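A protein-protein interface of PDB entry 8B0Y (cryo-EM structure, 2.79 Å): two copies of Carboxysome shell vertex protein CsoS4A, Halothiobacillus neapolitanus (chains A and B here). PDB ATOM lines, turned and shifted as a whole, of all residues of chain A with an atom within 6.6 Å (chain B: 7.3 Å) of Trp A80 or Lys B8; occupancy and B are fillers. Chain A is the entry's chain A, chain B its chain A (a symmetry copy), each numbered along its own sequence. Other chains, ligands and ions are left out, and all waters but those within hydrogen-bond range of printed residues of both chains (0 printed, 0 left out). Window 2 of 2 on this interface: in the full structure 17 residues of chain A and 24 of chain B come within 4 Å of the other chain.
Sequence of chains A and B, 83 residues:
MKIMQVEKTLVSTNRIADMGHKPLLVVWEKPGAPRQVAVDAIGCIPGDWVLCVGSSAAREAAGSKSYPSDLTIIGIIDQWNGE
No position is printed for both chains.
Among the printed residues, pairs that only touch across the chains: Trp A80 with Lys B8 (3.4 Å), Ile A3 with Leu B10 (3.6 Å), Ile A3 with Val B37 (3.7 Å), Ile A77 with Leu B10 (3.7 Å) and Trp A80 with Arg B35 (3.8 Å).
Printed residues of chain B that touch a printed residue of chain A: Lys B8, Leu B10, Arg B35 and Val B37. Hydrophobic or aromatic side chains of chain B within 4 Å of the printed part of chain A: Leu B10 and Val B37. Along chain B the printed residues that touch a printed residue of chain A span positions 8 to 37. Of the 8 printed residues of chain A, 3 touch a printed residue of chain B. Along chain A the printed residues that touch a printed residue of chain B span positions 3 to 80. Among the printed residues, no Asp or Glu carboxylate lies within 4 Å of a Lys or Arg side-chain nitrogen of the other chain.
Of the printed residues of chain B, Ile A3 touches Leu B10 and Val B37. Trp A80 touches just these residues of chain B: Lys B8 (3.4 Å) and Arg B35 (3.8 Å). Glu B7 touches none of the printed residues of chain A. Lys B8 touches just one residue of chain A: Trp A80 (3.4 Å). Val B26 touches none of the printed residues of chain A. Of the printed residues of chain A, Arg B35 touches Trp A80 (3.8 Å). The nearest residue of chain B that does not touch Trp A80 is Leu B10 (4.1 Å). The nearest residue of chain A that does not touch Lys B8 is Asn A81 (6.3 Å). The nearest printed residue of chain B that does not touch Ile A3 is Val B26 (4.9 Å).
O of Trp A49 lies within hydrogen-bond range of N of Ile A77, 3.0 Å away. The side-chain carboxylate of Glu B7 lies within salt-bridge range of the side-chain amino group of Lys B8, at 3.5 Å. The side-chain carboxylate (OE1) of Glu B7 is in salt-bridge range of the guanidinium group (NE) of Arg B35. The backbone NH (N) of Val B26 is in hydrogen-bond range of the backbone carbonyl oxygen (O) of Lys B8. N of Leu B10 sits at hydrogen-bond distance from O of Leu B24 (2.9 Å).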
ATOM      1  N   ILE A   3      14.735 -22.578   7.612  1.00  0.00           N
ATOM      2  CA  ILE A   3      13.820 -23.469   8.312  1.00  0.00           C
ATOM      3  C   ILE A   3      13.368 -24.545   7.337  1.00  0.00           C
ATOM      4  O   ILE A   3      12.639 -24.261   6.379  1.00  0.00           O
ATOM      5  CB  ILE A   3      12.618 -22.706   8.886  1.00  0.00           C
ATOM      6  CG1 ILE A   3      13.093 -21.683   9.918  1.00  0.00           C
ATOM      7  CG2 ILE A   3      11.611 -23.671   9.485  1.00  0.00           C
ATOM      8  CD1 ILE A   3      12.074 -20.625  10.247  1.00  0.00           C
ATOM      9  N   GLU A  29      12.506 -27.299   2.583  1.00  0.00           N
ATOM     10  CA  GLU A  29      11.821 -26.148   3.161  1.00  0.00           C
ATOM     11  C   GLU A  29      10.343 -26.447   3.378  1.00  0.00           C
ATOM     12  O   GLU A  29       9.753 -26.028   4.381  1.00  0.00           O
ATOM     13  CB  GLU A  29      12.000 -24.925   2.264  1.00  0.00           C
ATOM     14  CG  GLU A  29      13.394 -24.323   2.312  1.00  0.00           C
ATOM     15  CD  GLU A  29      13.534 -23.108   1.416  1.00  0.00           C
ATOM     16  OE1 GLU A  29      12.593 -22.826   0.646  1.00  0.00           O
ATOM     17  OE2 GLU A  29      14.585 -22.436   1.481  1.00  0.00           O
ATOM     18  N   TRP A  49      10.063 -29.397  12.314  1.00  0.00           N
ATOM     19  CA  TRP A  49      10.542 -28.134  11.771  1.00  0.00           C
ATOM     20  C   TRP A  49      11.843 -27.786  12.479  1.00  0.00           C
ATOM     21  O   TRP A  49      11.846 -27.532  13.688  1.00  0.00           O
ATOM     22  CB  TRP A  49       9.506 -27.027  11.950  1.00  0.00           C
ATOM     23  CG  TRP A  49       8.318 -27.184  11.060  1.00  0.00           C
ATOM     24  CD1 TRP A  49       7.079 -27.620  11.419  1.00  0.00           C
ATOM     25  CD2 TRP A  49       8.258 -26.912   9.656  1.00  0.00           C
ATOM     26  NE1 TRP A  49       6.248 -27.634  10.326  1.00  0.00           N
ATOM     27  CE2 TRP A  49       6.949 -27.204   9.231  1.00  0.00           C
ATOM     28  CE3 TRP A  49       9.184 -26.448   8.718  1.00  0.00           C
ATOM     29  CZ2 TRP A  49       6.541 -27.048   7.910  1.00  0.00           C
ATOM     30  CZ3 TRP A  49       8.778 -26.294   7.408  1.00  0.00           C
ATOM     31  CH2 TRP A  49       7.469 -26.594   7.015  1.00  0.00           C
ATOM     32  N   ILE A  77      12.720 -26.094  16.164  1.00  0.00           N
ATOM     33  CA  ILE A  77      11.921 -24.918  16.487  1.00  0.00           C
ATOM     34  C   ILE A  77      10.768 -25.331  17.391  1.00  0.00           C
ATOM     35  O   ILE A  77      10.030 -26.275  17.085  1.00  0.00           O
ATOM     36  CB  ILE A  77      11.416 -24.236  15.209  1.00  0.00           C
ATOM     37  CG1 ILE A  77      12.589 -23.958  14.271  1.00  0.00           C
ATOM     38  CG2 ILE A  77      10.687 -22.947  15.545  1.00  0.00           C
ATOM     39  CD1 ILE A  77      12.188 -23.295  12.992  1.00  0.00           C
ATOM     40  N   ASP A  78      10.615 -24.621  18.510  1.00  0.00           N
ATOM     41  CA  ASP A  78       9.600 -24.982  19.494  1.00  0.00           C
ATOM     42  C   ASP A  78       8.195 -24.859  18.916  1.00  0.00           C
ATOM     43  O   ASP A  78       7.342 -25.722  19.147  1.00  0.00           O
ATOM     44  CB  ASP A  78       9.748 -24.109  20.741  1.00  0.00           C
ATOM     45  CG  ASP A  78      11.048 -24.360  21.477  1.00  0.00           C
ATOM     46  OD1 ASP A  78      11.835 -25.214  21.019  1.00  0.00           O
ATOM     47  OD2 ASP A  78      11.281 -23.707  22.515  1.00  0.00           O
ATOM     48  N   GLN A  79       7.934 -23.791  18.165  1.00  0.00           N
ATOM     49  CA  GLN A  79       6.615 -23.541  17.596  1.00  0.00           C
ATOM     50  C   GLN A  79       6.769 -23.076  16.157  1.00  0.00           C
ATOM     51  O   GLN A  79       7.240 -21.962  15.910  1.00  0.00           O
ATOM     52  CB  GLN A  79       5.850 -22.498  18.416  1.00  0.00           C
ATOM     53  CG  GLN A  79       4.700 -23.069  19.229  1.00  0.00           C
ATOM     54  CD  GLN A  79       5.151 -23.636  20.562  1.00  0.00           C
ATOM     55  OE1 GLN A  79       5.745 -22.933  21.380  1.00  0.00           O
ATOM     56  NE2 GLN A  79       4.870 -24.914  20.786  1.00  0.00           N
ATOM     57  N   TRP A  80       6.369 -23.927  15.215  1.00  0.00           N
ATOM     58  CA  TRP A  80       6.365 -23.573  13.804  1.00  0.00           C
ATOM     59  C   TRP A  80       5.293 -24.392  13.103  1.00  0.00           C
ATOM     60  O   TRP A  80       4.867 -25.442  13.592  1.00  0.00           O
ATOM     61  CB  TRP A  80       7.735 -23.804  13.156  1.00  0.00           C
ATOM     62  CG  TRP A  80       7.910 -23.074  11.860  1.00  0.00           C
ATOM     63  CD1 TRP A  80       7.779 -23.592  10.606  1.00  0.00           C
ATOM     64  CD2 TRP A  80       8.239 -21.691  11.689  1.00  0.00           C
ATOM     65  NE1 TRP A  80       8.008 -22.621   9.665  1.00  0.00           N
ATOM     66  CE2 TRP A  80       8.293 -21.444  10.304  1.00  0.00           C
ATOM     67  CE3 TRP A  80       8.494 -20.638  12.571  1.00  0.00           C
ATOM     68  CZ2 TRP A  80       8.591 -20.187   9.781  1.00  0.00           C
ATOM     69  CZ3 TRP A  80       8.791 -19.393  12.051  1.00  0.00           C
ATOM     70  CH2 TRP A  80       8.837 -19.177  10.670  1.00  0.00           C
ATOM     71  N   ASN A  81       4.861 -23.898  11.947  1.00  0.00           N
ATOM     72  CA  ASN A  81       3.830 -24.570  11.167  1.00  0.00           C
ATOM     73  C   ASN A  81       3.994 -24.309   9.672  1.00  0.00           C
ATOM     74  O   ASN A  81       4.619 -23.330   9.267  1.00  0.00           O
ATOM     75  CB  ASN A  81       2.440 -24.128  11.629  1.00  0.00           C
ATOM     76  CG  ASN A  81       2.291 -22.618  11.674  1.00  0.00           C
ATOM     77  OD1 ASN A  81       3.209 -21.881  11.316  1.00  0.00           O
ATOM     78  ND2 ASN A  81       1.129 -22.152  12.116  1.00  0.00           N
ATOM     79  N   GLN B   5      14.042  -7.382   6.198  1.00  0.00           N
ATOM     80  CA  GLN B   5      13.157  -6.816   7.205  1.00  0.00           C
ATOM     81  C   GLN B   5      12.882  -7.864   8.272  1.00  0.00           C
ATOM     82  O   GLN B   5      12.587  -9.020   7.949  1.00  0.00           O
ATOM     83  CB  GLN B   5      11.847  -6.339   6.576  1.00  0.00           C
ATOM     84  CG  GLN B   5      11.016  -5.445   7.478  1.00  0.00           C
ATOM     85  CD  GLN B   5       9.735  -4.982   6.818  1.00  0.00           C
ATOM     86  OE1 GLN B   5       9.149  -5.695   6.004  1.00  0.00           O
ATOM     87  NE2 GLN B   5       9.295  -3.779   7.160  1.00  0.00           N
ATOM     88  N   VAL B   6      12.986  -7.465   9.534  1.00  0.00           N
ATOM     89  CA  VAL B   6      12.734  -8.374  10.646  1.00  0.00           C
ATOM     90  C   VAL B   6      11.234  -8.617  10.746  1.00  0.00           C
ATOM     91  O   VAL B   6      10.442  -7.671  10.781  1.00  0.00           O
ATOM     92  CB  VAL B   6      13.292  -7.812  11.961  1.00  0.00           C
ATOM     93  CG1 VAL B   6      13.037  -8.782  13.103  1.00  0.00           C
ATOM     94  CG2 VAL B   6      14.776  -7.522  11.821  1.00  0.00           C
ATOM     95  N   GLU B   7      10.841  -9.890  10.783  1.00  0.00           N
ATOM     96  CA  GLU B   7       9.430 -10.249  10.900  1.00  0.00           C
ATOM     97  C   GLU B   7       9.048 -10.577  12.339  1.00  0.00           C
ATOM     98  O   GLU B   7       8.102 -10.000  12.885  1.00  0.00           O
ATOM     99  CB  GLU B   7       9.109 -11.434   9.985  1.00  0.00           C
ATOM    100  CG  GLU B   7       7.647 -11.843  10.022  1.00  0.00           C
ATOM    101  CD  GLU B   7       7.419 -13.235   9.478  1.00  0.00           C
ATOM    102  OE1 GLU B   7       8.397 -13.868   9.034  1.00  0.00           O
ATOM    103  OE2 GLU B   7       6.259 -13.696   9.496  1.00  0.00           O
ATOM    104  N   LYS B   8       9.771 -11.505  12.962  1.00  0.00           N
ATOM    105  CA  LYS B   8       9.450 -11.953  14.308  1.00  0.00           C
ATOM    106  C   LYS B   8      10.659 -12.675  14.882  1.00  0.00           C
ATOM    107  O   LYS B   8      11.654 -12.908  14.193  1.00  0.00           O
ATOM    108  CB  LYS B   8       8.211 -12.854  14.316  1.00  0.00           C
ATOM    109  CG  LYS B   8       8.475 -14.275  13.855  1.00  0.00           C
ATOM    110  CD  LYS B   8       7.481 -14.700  12.790  1.00  0.00           C
ATOM    111  CE  LYS B   8       7.581 -16.187  12.507  1.00  0.00           C
ATOM    112  NZ  LYS B   8       6.659 -16.610  11.419  1.00  0.00           N
ATOM    113  N   THR B   9      10.560 -13.019  16.162  1.00  0.00           N
ATOM    114  CA  THR B   9      11.608 -13.755  16.848  1.00  0.00           C
ATOM    115  C   THR B   9      11.405 -15.256  16.674  1.00  0.00           C
ATOM    116  O   THR B   9      10.304 -15.732  16.390  1.00  0.00           O
ATOM    117  CB  THR B   9      11.633 -13.404  18.337  1.00  0.00           C
ATOM    118  OG1 THR B   9      10.401 -13.810  18.944  1.00  0.00           O
ATOM    119  CG2 THR B   9      11.807 -11.910  18.529  1.00  0.00           C
ATOM    120  N   LEU B  10      12.492 -16.003  16.850  1.00  0.00           N
ATOM    121  CA  LEU B  10      12.461 -17.458  16.779  1.00  0.00           C
ATOM    122  C   LEU B  10      13.161 -18.025  18.002  1.00  0.00           C
ATOM    123  O   LEU B  10      14.272 -17.604  18.335  1.00  0.00           O
ATOM    124  CB  LEU B  10      13.126 -17.963  15.492  1.00  0.00           C
ATOM    125  CG  LEU B  10      12.979 -19.452  15.175  1.00  0.00           C
ATOM    126  CD1 LEU B  10      12.575 -19.645  13.726  1.00  0.00           C
ATOM    127  CD2 LEU B  10      14.273 -20.190  15.466  1.00  0.00           C
ATOM    128  N   LEU B  24      17.641 -15.135  17.986  1.00  0.00           N
ATOM    129  CA  LEU B  24      17.380 -15.517  16.607  1.00  0.00           C
ATOM    130  C   LEU B  24      16.156 -14.771  16.097  1.00  0.00           C
ATOM    131  O   LEU B  24      15.135 -14.696  16.786  1.00  0.00           O
ATOM    132  CB  LEU B  24      17.161 -17.027  16.479  1.00  0.00           C
ATOM    133  CG  LEU B  24      18.324 -17.920  16.906  1.00  0.00           C
ATOM    134  CD1 LEU B  24      17.926 -19.382  16.820  1.00  0.00           C
ATOM    135  CD2 LEU B  24      19.551 -17.643  16.054  1.00  0.00           C
ATOM    136  N   LEU B  25      16.262 -14.222  14.890  1.00  0.00           N
ATOM    137  CA  LEU B  25      15.195 -13.433  14.294  1.00  0.00           C
ATOM    138  C   LEU B  25      14.831 -13.994  12.930  1.00  0.00           C
ATOM    139  O   LEU B  25      15.704 -14.417  12.170  1.00  0.00           O
ATOM    140  CB  LEU B  25      15.601 -11.963  14.145  1.00  0.00           C
ATOM    141  CG  LEU B  25      15.780 -11.154  15.426  1.00  0.00           C
ATOM    142  CD1 LEU B  25      16.227  -9.753  15.084  1.00  0.00           C
ATOM    143  CD2 LEU B  25      14.494 -11.121  16.221  1.00  0.00           C
ATOM    144  N   VAL B  26      13.538 -13.987  12.625  1.00  0.00           N
ATOM    145  CA  VAL B  26      13.064 -14.368  11.301  1.00  0.00           C
ATOM    146  C   VAL B  26      13.065 -13.136  10.407  1.00  0.00           C
ATOM    147  O   VAL B  26      12.425 -12.127  10.722  1.00  0.00           O
ATOM    148  CB  VAL B  26      11.665 -14.997  11.382  1.00  0.00           C
ATOM    149  CG1 VAL B  26      11.181 -15.380   9.998  1.00  0.00           C
ATOM    150  CG2 VAL B  26      11.681 -16.210  12.299  1.00  0.00           C
ATOM    151  N   VAL B  27      13.786 -13.213   9.292  1.00  0.00           N
ATOM    152  CA  VAL B  27      13.966 -12.077   8.400  1.00  0.00           C
ATOM    153  C   VAL B  27      13.610 -12.486   6.979  1.00  0.00           C
ATOM    154  O   VAL B  27      13.720 -13.656   6.599  1.00  0.00           O
ATOM    155  CB  VAL B  27      15.409 -11.528   8.456  1.00  0.00           C
ATOM    156  CG1 VAL B  27      15.669 -10.840   9.785  1.00  0.00           C
ATOM    157  CG2 VAL B  27      16.412 -12.644   8.228  1.00  0.00           C
ATOM    158  N   TRP B  28      13.168 -11.508   6.194  1.00  0.00           N
ATOM    159  CA  TRP B  28      12.956 -11.674   4.765  1.00  0.00           C
ATOM    160  C   TRP B  28      13.309 -10.375   4.059  1.00  0.00           C
ATOM    161  O   TRP B  28      13.317  -9.301   4.664  1.00  0.00           O
ATOM    162  CB  TRP B  28      11.509 -12.064   4.421  1.00  0.00           C
ATOM    163  CG  TRP B  28      10.451 -11.338   5.202  1.00  0.00           C
ATOM    164  CD1 TRP B  28      10.529 -10.079   5.724  1.00  0.00           C
ATOM    165  CD2 TRP B  28       9.128 -11.806   5.486  1.00  0.00           C
ATOM    166  NE1 TRP B  28       9.353  -9.749   6.346  1.00  0.00           N
ATOM    167  CE2 TRP B  28       8.472 -10.790   6.211  1.00  0.00           C
ATOM    168  CE3 TRP B  28       8.436 -12.990   5.210  1.00  0.00           C
ATOM    169  CZ2 TRP B  28       7.163 -10.923   6.663  1.00  0.00           C
ATOM    170  CZ3 TRP B  28       7.138 -13.118   5.660  1.00  0.00           C
ATOM    171  CH2 TRP B  28       6.515 -12.092   6.379  1.00  0.00           C
ATOM    172  N   ARG B  35      11.418 -17.017   4.024  1.00  0.00           N
ATOM    173  CA  ARG B  35      11.849 -16.672   5.369  1.00  0.00           C
ATOM    174  C   ARG B  35      13.252 -17.198   5.642  1.00  0.00           C
ATOM    175  O   ARG B  35      13.670 -18.228   5.107  1.00  0.00           O
ATOM    176  CB  ARG B  35      10.876 -17.238   6.403  1.00  0.00           C
ATOM    177  CG  ARG B  35       9.521 -16.556   6.419  1.00  0.00           C
ATOM    178  CD  ARG B  35       8.782 -16.849   7.712  1.00  0.00           C
ATOM    179  NE  ARG B  35       7.486 -16.187   7.767  1.00  0.00           N
ATOM    180  CZ  ARG B  35       6.385 -16.646   7.192  1.00  0.00           C
ATOM    181  NH1 ARG B  35       6.386 -17.778   6.505  1.00  0.00           N
ATOM    182  NH2 ARG B  35       5.256 -15.956   7.306  1.00  0.00           N
ATOM    183  N   GLN B  36      13.978 -16.473   6.488  1.00  0.00           N
ATOM    184  CA  GLN B  36      15.310 -16.873   6.912  1.00  0.00           C
ATOM    185  C   GLN B  36      15.489 -16.503   8.374  1.00  0.00           C
ATOM    186  O   GLN B  36      14.802 -15.628   8.902  1.00  0.00           O
ATOM    187  CB  GLN B  36      16.400 -16.216   6.058  1.00  0.00           C
ATOM    188  CG  GLN B  36      16.750 -16.990   4.803  1.00  0.00           C
ATOM    189  CD  GLN B  36      17.441 -16.132   3.769  1.00  0.00           C
ATOM    190  OE1 GLN B  36      18.669 -16.071   3.717  1.00  0.00           O
ATOM    191  NE2 GLN B  36      16.656 -15.453   2.942  1.00  0.00           N
ATOM    192  N   VAL B  37      16.424 -17.184   9.029  1.00  0.00           N
ATOM    193  CA  VAL B  37      16.720 -16.971  10.439  1.00  0.00           C
ATOM    194  C   VAL B  37      18.133 -16.419  10.548  1.00  0.00           C
ATOM    195  O   VAL B  37      19.074 -16.993   9.987  1.00  0.00           O
ATOM    196  CB  VAL B  37      16.569 -18.268  11.255  1.00  0.00           C
ATOM    197  CG1 VAL B  37      16.821 -18.002  12.729  1.00  0.00           C
ATOM    198  CG2 VAL B  37      15.189 -18.863  11.043  1.00  0.00           C
ATOM    199  N   ILE B  45      13.759  -4.577  16.362  1.00  0.00           N
ATOM    200  CA  ILE B  45      12.353  -4.923  16.551  1.00  0.00           C
ATOM    201  C   ILE B  45      11.758  -5.342  15.211  1.00  0.00           C
ATOM    202  O   ILE B  45      12.329  -5.018  14.159  1.00  0.00           O
ATOM    203  CB  ILE B  45      11.578  -3.747  17.167  1.00  0.00           C
ATOM    204  CG1 ILE B  45      11.759  -2.490  16.316  1.00  0.00           C
ATOM    205  CG2 ILE B  45      12.037  -3.501  18.594  1.00  0.00           C
ATOM    206  CD1 ILE B  45      11.415  -1.203  17.036  1.00  0.00           C
ATOM    207  N   PRO B  46      10.644  -6.072  15.196  1.00  0.00           N
ATOM    208  CA  PRO B  46      10.012  -6.424  13.918  1.00  0.00           C
ATOM    209  C   PRO B  46       9.637  -5.186  13.117  1.00  0.00           C
ATOM    210  O   PRO B  46       9.233  -4.161  13.671  1.00  0.00           O
ATOM    211  CB  PRO B  46       8.773  -7.215  14.344  1.00  0.00           C
ATOM    212  CG  PRO B  46       9.146  -7.796  15.656  1.00  0.00           C
ATOM    213  CD  PRO B  46      10.009  -6.768  16.329  1.00  0.00           C
ATOM    214  N   GLY B  47       9.776  -5.294  11.797  1.00  0.00           N
ATOM    215  CA  GLY B  47       9.560  -4.179  10.904  1.00  0.00           C
ATOM    216  C   GLY B  47      10.794  -3.357  10.609  1.00  0.00           C
ATOM    217  O   GLY B  47      10.744  -2.488   9.730  1.00  0.00           O
